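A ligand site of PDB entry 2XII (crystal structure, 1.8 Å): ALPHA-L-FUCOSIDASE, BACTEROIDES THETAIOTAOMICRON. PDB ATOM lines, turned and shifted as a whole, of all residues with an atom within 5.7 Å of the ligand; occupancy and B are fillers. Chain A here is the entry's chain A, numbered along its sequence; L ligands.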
ATOM      1  N   PHE A  33      27.532  -7.591   9.050  1.00  0.00           N
ATOM      2  CA  PHE A  33      26.875  -6.680   8.129  1.00  0.00           C
ATOM      3  C   PHE A  33      25.534  -7.367   7.753  1.00  0.00           C
ATOM      4  O   PHE A  33      25.490  -8.582   7.510  1.00  0.00           O
ATOM      5  CB  PHE A  33      27.725  -6.518   6.844  1.00  0.00           C
ATOM      6  CG  PHE A  33      27.916  -5.113   6.380  1.00  0.00           C
ATOM      7  CD1 PHE A  33      29.163  -4.706   5.894  1.00  0.00           C
ATOM      8  CD2 PHE A  33      26.877  -4.195   6.407  1.00  0.00           C
ATOM      9  CE1 PHE A  33      29.367  -3.424   5.474  1.00  0.00           C
ATOM     10  CE2 PHE A  33      27.084  -2.877   6.016  1.00  0.00           C
ATOM     11  CZ  PHE A  33      28.329  -2.498   5.520  1.00  0.00           C
ATOM     12  N   HIS A  35      22.712  -6.712   4.852  1.00  0.00           N
ATOM     13  CA  HIS A  35      22.118  -6.044   3.703  1.00  0.00           C
ATOM     14  C   HIS A  35      20.747  -6.651   3.504  1.00  0.00           C
ATOM     15  O   HIS A  35      20.635  -7.810   3.077  1.00  0.00           O
ATOM     16  CB  HIS A  35      22.947  -6.249   2.417  1.00  0.00           C
ATOM     17  CG  HIS A  35      24.124  -5.326   2.305  1.00  0.00           C
ATOM     18  ND1 HIS A  35      25.267  -5.480   3.056  1.00  0.00           N
ATOM     19  CD2 HIS A  35      24.344  -4.276   1.476  1.00  0.00           C
ATOM     20  CE1 HIS A  35      26.130  -4.524   2.729  1.00  0.00           C
ATOM     21  NE2 HIS A  35      25.616  -3.804   1.746  1.00  0.00           N
ATOM     22  N   GLU A  56      21.928  -6.788  -4.872  1.00  0.00           N
ATOM     23  CA  GLU A  56      21.422  -5.503  -4.382  1.00  0.00           C
ATOM     24  C   GLU A  56      21.512  -4.392  -5.435  1.00  0.00           C
ATOM     25  O   GLU A  56      20.903  -3.339  -5.277  1.00  0.00           O
ATOM     26  CB  GLU A  56      22.099  -5.113  -3.077  1.00  0.00           C
ATOM     27  CG  GLU A  56      23.545  -4.621  -3.133  1.00  0.00           C
ATOM     28  CD  GLU A  56      24.616  -5.694  -3.395  1.00  0.00           C
ATOM     29  OE1 GLU A  56      24.327  -6.895  -3.467  1.00  0.00           O
ATOM     30  OE2 GLU A  56      25.793  -5.292  -3.497  1.00  0.00           O
ATOM     31  N   TRP A  57      22.234  -4.682  -6.518  1.00  0.00           N
ATOM     32  CA  TRP A  57      22.332  -3.820  -7.714  1.00  0.00           C
ATOM     33  C   TRP A  57      21.439  -4.299  -8.879  1.00  0.00           C
ATOM     34  O   TRP A  57      21.641  -3.835 -10.014  1.00  0.00           O
ATOM     35  CB  TRP A  57      23.783  -3.763  -8.210  1.00  0.00           C
ATOM     36  CG  TRP A  57      24.662  -2.811  -7.443  1.00  0.00           C
ATOM     37  CD1 TRP A  57      25.232  -3.033  -6.222  1.00  0.00           C
ATOM     38  CD2 TRP A  57      25.146  -1.537  -7.890  1.00  0.00           C
ATOM     39  NE1 TRP A  57      26.014  -1.965  -5.852  1.00  0.00           N
ATOM     40  CE2 TRP A  57      25.967  -1.022  -6.849  1.00  0.00           C
ATOM     41  CE3 TRP A  57      24.942  -0.769  -9.042  1.00  0.00           C
ATOM     42  CZ2 TRP A  57      26.577   0.230  -6.926  1.00  0.00           C
ATOM     43  CZ3 TRP A  57      25.570   0.470  -9.127  1.00  0.00           C
ATOM     44  CH2 TRP A  57      26.385   0.953  -8.084  1.00  0.00           C
ATOM     45  N   HIS A 104      19.575   1.276   1.331  1.00  0.00           N
ATOM     46  CA  HIS A 104      20.632   0.977   0.377  1.00  0.00           C
ATOM     47  C   HIS A 104      20.454   1.916  -0.829  1.00  0.00           C
ATOM     48  O   HIS A 104      19.690   2.874  -0.749  1.00  0.00           O
ATOM     49  CB  HIS A 104      20.638  -0.496  -0.033  1.00  0.00           C
ATOM     50  CG  HIS A 104      21.967  -0.936  -0.535  1.00  0.00           C
ATOM     51  ND1 HIS A 104      22.276  -1.000  -1.883  1.00  0.00           N
ATOM     52  CD2 HIS A 104      23.102  -1.276   0.113  1.00  0.00           C
ATOM     53  CE1 HIS A 104      23.536  -1.382  -2.025  1.00  0.00           C
ATOM     54  NE2 HIS A 104      24.057  -1.550  -0.829  1.00  0.00           N
ATOM     55  N   HIS A 105      21.152   1.661  -1.944  1.00  0.00           N
ATOM     56  CA  HIS A 105      21.075   2.580  -3.122  1.00  0.00           C
ATOM     57  C   HIS A 105      19.650   2.730  -3.649  1.00  0.00           C
ATOM     58  O   HIS A 105      19.256   3.809  -4.123  1.00  0.00           O
ATOM     59  CB  HIS A 105      22.018   2.118  -4.262  1.00  0.00           C
ATOM     60  CG  HIS A 105      23.409   1.803  -3.821  1.00  0.00           C
ATOM     61  ND1 HIS A 105      24.077   2.535  -2.844  1.00  0.00           N
ATOM     62  CD2 HIS A 105      24.279   0.861  -4.239  1.00  0.00           C
ATOM     63  CE1 HIS A 105      25.278   2.022  -2.684  1.00  0.00           C
ATOM     64  NE2 HIS A 105      25.428   1.019  -3.519  1.00  0.00           N
ATOM     65  N   TYR A 147      24.414   1.609   8.412  1.00  0.00           N
ATOM     66  CA  TYR A 147      24.837   1.827   7.044  1.00  0.00           C
ATOM     67  C   TYR A 147      23.808   2.769   6.429  1.00  0.00           C
ATOM     68  O   TYR A 147      22.590   2.579   6.574  1.00  0.00           O
ATOM     69  CB  TYR A 147      24.832   0.494   6.294  1.00  0.00           C
ATOM     70  CG  TYR A 147      25.008   0.607   4.787  1.00  0.00           C
ATOM     71  CD1 TYR A 147      26.144   0.102   4.168  1.00  0.00           C
ATOM     72  CD2 TYR A 147      24.028   1.178   3.994  1.00  0.00           C
ATOM     73  CE1 TYR A 147      26.294   0.204   2.776  1.00  0.00           C
ATOM     74  CE2 TYR A 147      24.174   1.298   2.638  1.00  0.00           C
ATOM     75  CZ  TYR A 147      25.303   0.805   2.037  1.00  0.00           C
ATOM     76  OH  TYR A 147      25.422   0.964   0.680  1.00  0.00           O
ATOM     77  N   TRP A 196      27.932   4.593   8.877  1.00  0.00           N
ATOM     78  CA  TRP A 196      28.865   4.114   7.884  1.00  0.00           C
ATOM     79  C   TRP A 196      28.286   4.499   6.549  1.00  0.00           C
ATOM     80  O   TRP A 196      27.348   3.873   6.066  1.00  0.00           O
ATOM     81  CB  TRP A 196      29.035   2.614   8.024  1.00  0.00           C
ATOM     82  CG  TRP A 196      30.212   2.020   7.305  1.00  0.00           C
ATOM     83  CD1 TRP A 196      31.470   1.848   7.793  1.00  0.00           C
ATOM     84  CD2 TRP A 196      30.222   1.511   5.960  1.00  0.00           C
ATOM     85  NE1 TRP A 196      32.263   1.237   6.853  1.00  0.00           N
ATOM     86  CE2 TRP A 196      31.513   0.999   5.724  1.00  0.00           C
ATOM     87  CE3 TRP A 196      29.270   1.402   4.955  1.00  0.00           C
ATOM     88  CZ2 TRP A 196      31.871   0.423   4.528  1.00  0.00           C
ATOM     89  CZ3 TRP A 196      29.631   0.789   3.761  1.00  0.00           C
ATOM     90  CH2 TRP A 196      30.914   0.332   3.559  1.00  0.00           C
ATOM     91  N   ASP A 198      27.987   5.176   2.549  1.00  0.00           N
ATOM     92  CA  ASP A 198      28.357   4.511   1.332  1.00  0.00           C
ATOM     93  C   ASP A 198      27.689   5.253   0.174  1.00  0.00           C
ATOM     94  O   ASP A 198      26.869   6.151   0.411  1.00  0.00           O
ATOM     95  CB  ASP A 198      27.919   3.069   1.418  1.00  0.00           C
ATOM     96  CG  ASP A 198      28.619   2.166   0.445  1.00  0.00           C
ATOM     97  OD1 ASP A 198      29.659   2.600  -0.103  1.00  0.00           O
ATOM     98  OD2 ASP A 198      28.131   1.037   0.228  1.00  0.00           O
ATOM     99  N   GLY A 199      28.045   4.929  -1.061  1.00  0.00           N
ATOM    100  CA  GLY A 199      27.485   5.641  -2.208  1.00  0.00           C
ATOM    101  C   GLY A 199      27.802   7.130  -2.170  1.00  0.00           C
ATOM    102  O   GLY A 199      26.942   7.953  -2.448  1.00  0.00           O
ATOM    103  N   THR A 200      29.035   7.455  -1.810  1.00  0.00           N
ATOM    104  CA  THR A 200      29.471   8.839  -1.692  1.00  0.00           C
ATOM    105  C   THR A 200      30.471   9.191  -2.795  1.00  0.00           C
ATOM    106  O   THR A 200      31.053  10.277  -2.755  1.00  0.00           O
ATOM    107  CB  THR A 200      30.178   9.098  -0.341  1.00  0.00           C
ATOM    108  OG1 THR A 200      31.260   8.178  -0.201  1.00  0.00           O
ATOM    109  CG2 THR A 200      29.208   8.951   0.855  1.00  0.00           C
ATOM    110  N   TRP A 201      30.647   8.302  -3.760  1.00  0.00           N
ATOM    111  CA  TRP A 201      31.704   8.429  -4.775  1.00  0.00           C
ATOM    112  C   TRP A 201      31.448   9.451  -5.887  1.00  0.00           C
ATOM    113  O   TRP A 201      32.341   9.732  -6.695  1.00  0.00           O
ATOM    114  CB  TRP A 201      32.019   7.081  -5.404  1.00  0.00           C
ATOM    115  CG  TRP A 201      30.819   6.365  -6.009  1.00  0.00           C
ATOM    116  CD1 TRP A 201      30.202   6.659  -7.177  1.00  0.00           C
ATOM    117  CD2 TRP A 201      30.135   5.246  -5.459  1.00  0.00           C
ATOM    118  NE1 TRP A 201      29.148   5.812  -7.385  1.00  0.00           N
ATOM    119  CE2 TRP A 201      29.094   4.920  -6.343  1.00  0.00           C
ATOM    120  CE3 TRP A 201      30.295   4.483  -4.294  1.00  0.00           C
ATOM    121  CZ2 TRP A 201      28.216   3.852  -6.124  1.00  0.00           C
ATOM    122  CZ3 TRP A 201      29.404   3.412  -4.072  1.00  0.00           C
ATOM    123  CH2 TRP A 201      28.385   3.124  -4.983  1.00  0.00           C
ATOM    124  N   ARG A 231      34.659   7.164   4.464  1.00  0.00           N
ATOM    125  CA  ARG A 231      34.031   7.173   3.156  1.00  0.00           C
ATOM    126  C   ARG A 231      33.143   8.408   2.922  1.00  0.00           C
ATOM    127  O   ARG A 231      33.014   8.867   1.802  1.00  0.00           O
ATOM    128  CB  ARG A 231      33.251   5.877   2.967  1.00  0.00           C
ATOM    129  CG  ARG A 231      33.255   5.395   1.591  1.00  0.00           C
ATOM    130  CD  ARG A 231      32.577   4.066   1.458  1.00  0.00           C
ATOM    131  NE  ARG A 231      33.457   2.964   1.794  1.00  0.00           N
ATOM    132  CZ  ARG A 231      33.257   1.723   1.373  1.00  0.00           C
ATOM    133  NH1 ARG A 231      32.183   1.423   0.622  1.00  0.00           N
ATOM    134  NH2 ARG A 231      34.111   0.766   1.701  1.00  0.00           N
ATOM    135  N   HIS A 241      38.721  11.075   1.948  1.00  0.00           N
ATOM    136  CA  HIS A 241      39.148  10.080   2.946  1.00  0.00           C
ATOM    137  C   HIS A 241      40.278  10.518   3.865  1.00  0.00           C
ATOM    138  O   HIS A 241      40.112  10.509   5.085  1.00  0.00           O
ATOM    139  CB  HIS A 241      39.475   8.750   2.289  1.00  0.00           C
ATOM    140  CG  HIS A 241      38.509   8.388   1.217  1.00  0.00           C
ATOM    141  ND1 HIS A 241      38.910   7.973  -0.032  1.00  0.00           N
ATOM    142  CD2 HIS A 241      37.161   8.462   1.182  1.00  0.00           C
ATOM    143  CE1 HIS A 241      37.840   7.746  -0.778  1.00  0.00           C
ATOM    144  NE2 HIS A 241      36.762   8.029  -0.062  1.00  0.00           N
ATOM    145  N   SER A 254      37.965   3.179   5.974  1.00  0.00           N
ATOM    146  CA  SER A 254      36.921   2.212   5.584  1.00  0.00           C
ATOM    147  C   SER A 254      36.982   1.719   4.142  1.00  0.00           C
ATOM    148  O   SER A 254      35.990   1.287   3.614  1.00  0.00           O
ATOM    149  CB  SER A 254      35.518   2.803   5.888  1.00  0.00           C
ATOM    150  OG  SER A 254      35.333   4.035   5.217  1.00  0.00           O
ATOM    151  N   GLY A 255      38.149   1.712   3.529  1.00  0.00           N
ATOM    152  CA  GLY A 255      38.264   1.330   2.126  1.00  0.00           C
ATOM    153  C   GLY A 255      38.588  -0.140   1.853  1.00  0.00           C
ATOM    154  O   GLY A 255      38.555  -0.568   0.697  1.00  0.00           O
ATOM    155  N   GLU A 257      37.298  -3.064   1.451  1.00  0.00           N
ATOM    156  CA  GLU A 257      36.066  -3.772   1.136  1.00  0.00           C
ATOM    157  C   GLU A 257      36.363  -4.924   0.202  1.00  0.00           C
ATOM    158  O   GLU A 257      36.873  -4.737  -0.928  1.00  0.00           O
ATOM    159  CB  GLU A 257      35.058  -2.781   0.576  1.00  0.00           C
ATOM    160  CG  GLU A 257      33.803  -3.372   0.049  1.00  0.00           C
ATOM    161  CD  GLU A 257      32.729  -2.372  -0.347  1.00  0.00           C
ATOM    162  OE1 GLU A 257      32.584  -1.339   0.337  1.00  0.00           O
ATOM    163  OE2 GLU A 257      32.025  -2.653  -1.347  1.00  0.00           O
ATOM    164  N   ARG A 258      36.120  -6.139   0.698  1.00  0.00           N
ATOM    165  CA  ARG A 258      36.463  -7.384  -0.025  1.00  0.00           C
ATOM    166  C   ARG A 258      37.963  -7.463  -0.347  1.00  0.00           C
ATOM    167  O   ARG A 258      38.393  -8.200  -1.255  1.00  0.00           O
ATOM    168  CB  ARG A 258      35.597  -7.584  -1.274  1.00  0.00           C
ATOM    169  CG  ARG A 258      34.079  -7.591  -1.004  1.00  0.00           C
ATOM    170  CD  ARG A 258      33.261  -7.955  -2.229  1.00  0.00           C
ATOM    171  NE  ARG A 258      33.569  -6.993  -3.292  1.00  0.00           N
ATOM    172  CZ  ARG A 258      34.198  -7.254  -4.429  1.00  0.00           C
ATOM    173  NH1 ARG A 258      34.561  -8.487  -4.784  1.00  0.00           N
ATOM    174  NH2 ARG A 258      34.439  -6.248  -5.245  1.00  0.00           N
ATOM    175  N   ARG A 259      38.769  -6.780   0.441  1.00  0.00           N
ATOM    176  CA  ARG A 259      40.207  -6.899   0.344  1.00  0.00           C
ATOM    177  C   ARG A 259      40.819  -6.439   1.641  1.00  0.00           C
ATOM    178  O   ARG A 259      40.140  -5.824   2.482  1.00  0.00           O
ATOM    179  CB  ARG A 259      40.756  -6.122  -0.837  1.00  0.00           C
ATOM    180  CG  ARG A 259      40.442  -4.680  -0.844  1.00  0.00           C
ATOM    181  CD  ARG A 259      40.834  -4.064  -2.205  1.00  0.00           C
ATOM    182  NE  ARG A 259      42.039  -3.246  -2.099  1.00  0.00           N
ATOM    183  CZ  ARG A 259      42.062  -1.949  -1.777  1.00  0.00           C
ATOM    184  NH1 ARG A 259      40.935  -1.288  -1.495  1.00  0.00           N
ATOM    185  NH2 ARG A 259      43.225  -1.307  -1.708  1.00  0.00           N
ATOM    186  N   CYS A 277      35.414  -4.851   5.503  1.00  0.00           N
ATOM    187  CA  CYS A 277      34.219  -5.633   5.350  1.00  0.00           C
ATOM    188  C   CYS A 277      34.395  -6.653   4.251  1.00  0.00           C
ATOM    189  O   CYS A 277      35.259  -6.505   3.377  1.00  0.00           O
ATOM    190  CB  CYS A 277      32.990  -4.751   5.132  1.00  0.00           C
ATOM    191  SG  CYS A 277      33.067  -3.616   3.719  1.00  0.00           S
ATOM    192  N   TRP A 285      26.159  -8.922  -1.659  1.00  0.00           N
ATOM    193  CA  TRP A 285      25.814  -8.411  -0.343  1.00  0.00           C
ATOM    194  C   TRP A 285      24.358  -8.739   0.028  1.00  0.00           C
ATOM    195  O   TRP A 285      24.081  -9.343   1.052  1.00  0.00           O
ATOM    196  CB  TRP A 285      26.105  -6.917  -0.240  1.00  0.00           C
ATOM    197  CG  TRP A 285      27.573  -6.553  -0.540  1.00  0.00           C
ATOM    198  CD1 TRP A 285      28.102  -6.307  -1.790  1.00  0.00           C
ATOM    199  CD2 TRP A 285      28.665  -6.385   0.386  1.00  0.00           C
ATOM    200  NE1 TRP A 285      29.433  -5.987  -1.685  1.00  0.00           N
ATOM    201  CE2 TRP A 285      29.808  -6.070  -0.365  1.00  0.00           C
ATOM    202  CE3 TRP A 285      28.792  -6.542   1.780  1.00  0.00           C
ATOM    203  CZ2 TRP A 285      31.047  -5.850   0.215  1.00  0.00           C
ATOM    204  CZ3 TRP A 285      30.003  -6.311   2.349  1.00  0.00           C
ATOM    205  CH2 TRP A 285      31.134  -5.982   1.562  1.00  0.00           C
HETATM  206  C1  LIG L   1      34.213   1.033  -2.479  1.00  0.00           C
HETATM  207  C2  LIG L   1      33.748   2.343  -2.304  1.00  0.00           C
HETATM  208  O1  LIG L   1      32.614   2.749  -2.570  1.00  0.00           O
HETATM  209  C3  LIG L   1      34.774   3.138  -1.827  1.00  0.00           C
HETATM  210  C4  LIG L   1      34.829   4.481  -1.472  1.00  0.00           C
HETATM  211  C5  LIG L   1      36.042   5.007  -0.980  1.00  0.00           C
HETATM  212  C6  LIG L   1      37.173   4.201  -0.855  1.00  0.00           C
HETATM  213  C7  LIG L   1      37.103   2.851  -1.217  1.00  0.00           C
HETATM  214  C8  LIG L   1      35.917   2.332  -1.714  1.00  0.00           C
HETATM  215  C9  LIG L   1      35.566   1.041  -2.132  1.00  0.00           C
HETATM  216  C10 LIG L   1      36.323  -0.129  -2.230  1.00  0.00           C
HETATM  217  C11 LIG L   1      35.738  -1.309  -2.664  1.00  0.00           C
HETATM  218  C12 LIG L   1      34.381  -1.325  -3.008  1.00  0.00           C
HETATM  219  C13 LIG L   1      33.622  -0.159  -2.919  1.00  0.00           C
HETATM  220  C14 LIG L   1      32.129  -0.269  -3.289  1.00  0.00           C
HETATM  221  O2  LIG L   1      31.769  -1.081  -4.140  1.00  0.00           O
HETATM  222  N1  LIG L   1      31.280   0.365  -2.480  1.00  0.00           N
HETATM  223  C15 LIG L   1      29.839   0.325  -2.645  1.00  0.00           C
HETATM  224  C16 LIG L   1      29.300  -1.009  -2.181  1.00  0.00           C
HETATM  225  N2  LIG L   1      29.531  -1.151  -0.729  1.00  0.00           N
HETATM  226  C17 LIG L   1      29.087  -2.530  -0.333  1.00  0.00           C
HETATM  227  C18 LIG L   1      29.284  -2.679   1.201  1.00  0.00           C
HETATM  228  C19 LIG L   1      27.663  -2.818  -0.741  1.00  0.00           C
HETATM  229  O3  LIG L   1      26.782  -1.994   0.012  1.00  0.00           O
HETATM  230  C20 LIG L   1      27.424  -2.546  -2.241  1.00  0.00           C
HETATM  231  O4  LIG L   1      26.046  -2.796  -2.560  1.00  0.00           O
HETATM  232  C21 LIG L   1      27.810  -1.106  -2.514  1.00  0.00           C
HETATM  233  O5  LIG L   1      27.597  -0.768  -3.912  1.00  0.00           O
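The side-chain carboxylate of Glu 56 lies within hydrogen-bond range of an oxygen (O4) of the ligand, 2.7 Å away.
NE2 of His 35 sits at hydrogen-bond distance from O3 of the ligand.
The side-chain carboxylate (OD2) of Asp 198 lies within salt-bridge range of a nitrogen (N2) of the ligand.
The side-chain hydroxyl (OH) of Tyr 147 lies within hydrogen-bond range of an oxygen (O3) of the ligand.
An oxygen (O3) of the ligand is in hydrogen-bond range of a ring nitrogen (NE2) of His 104, 2.9 Å away.
N2 of the ligand lies within salt-bridge range of OE2 of Glu 257, 3.0 Å away.
An oxygen (O1) of the ligand lies close to the guanidinium group (NH1) of Arg 231, 3.5 Å away.
A ring nitrogen (NE2) of His 105 is in hydrogen-bond range of an oxygen (O5) of the ligand (2.8 Å).
An oxygen (O5) of the ligand sits at hydrogen-bond distance from the indole nitrogen (NE1) of Trp 57.
The backbone carbonyl oxygen (O) of Arg 231 sits at hydrogen-bond distance from the side-chain hydroxyl (OG1) of Thr 200 (2.8 Å).
O of Gly 255 is in hydrogen-bond range of NH1 of Arg 259, at 3.3 Å.
A ring nitrogen (NE2) of His 104 sits at hydrogen-bond distance from the side-chain hydroxyl (OH) of Tyr 147 (3.2 Å).
OH of Tyr 147 is in hydrogen-bond range of OD2 of Asp 198 (2.7 Å).
The side-chain carboxylate (OD1) of Asp 198 is in salt-bridge range of the guanidinium group (NH1) of Arg 231 (2.9 Å).
OE1 of Glu 257 lies within salt-bridge range of NH1 of Arg 231, at 2.8 Å.
OE1 of Glu 56 lies within hydrogen-bond range of N of Trp 285.
The guanidinium group (NH2) of Arg 231 lies within hydrogen-bond range of the backbone carbonyl oxygen (O) of Ser 254, at 2.7 Å.
CE3 of Trp 201 touches O1 of the ligand, 3.4 Å away.
NE2 of His 241 touches C5 of the ligand, 3.2 Å away.
Gly 255 touches the ligand.
CE2 of Trp 285 touches C17 of the ligand (3.6 Å).
13 residues have an atom within 4 Å of the ligand: His 35, Glu 56, Trp 57, His 104, His 105, Tyr 147, Asp 198, Trp 201, Arg 231, His 241, Gly 255, Glu 257 and Trp 285.
Along chain A the residues within 4 Å of the ligand span positions 35 to 285.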
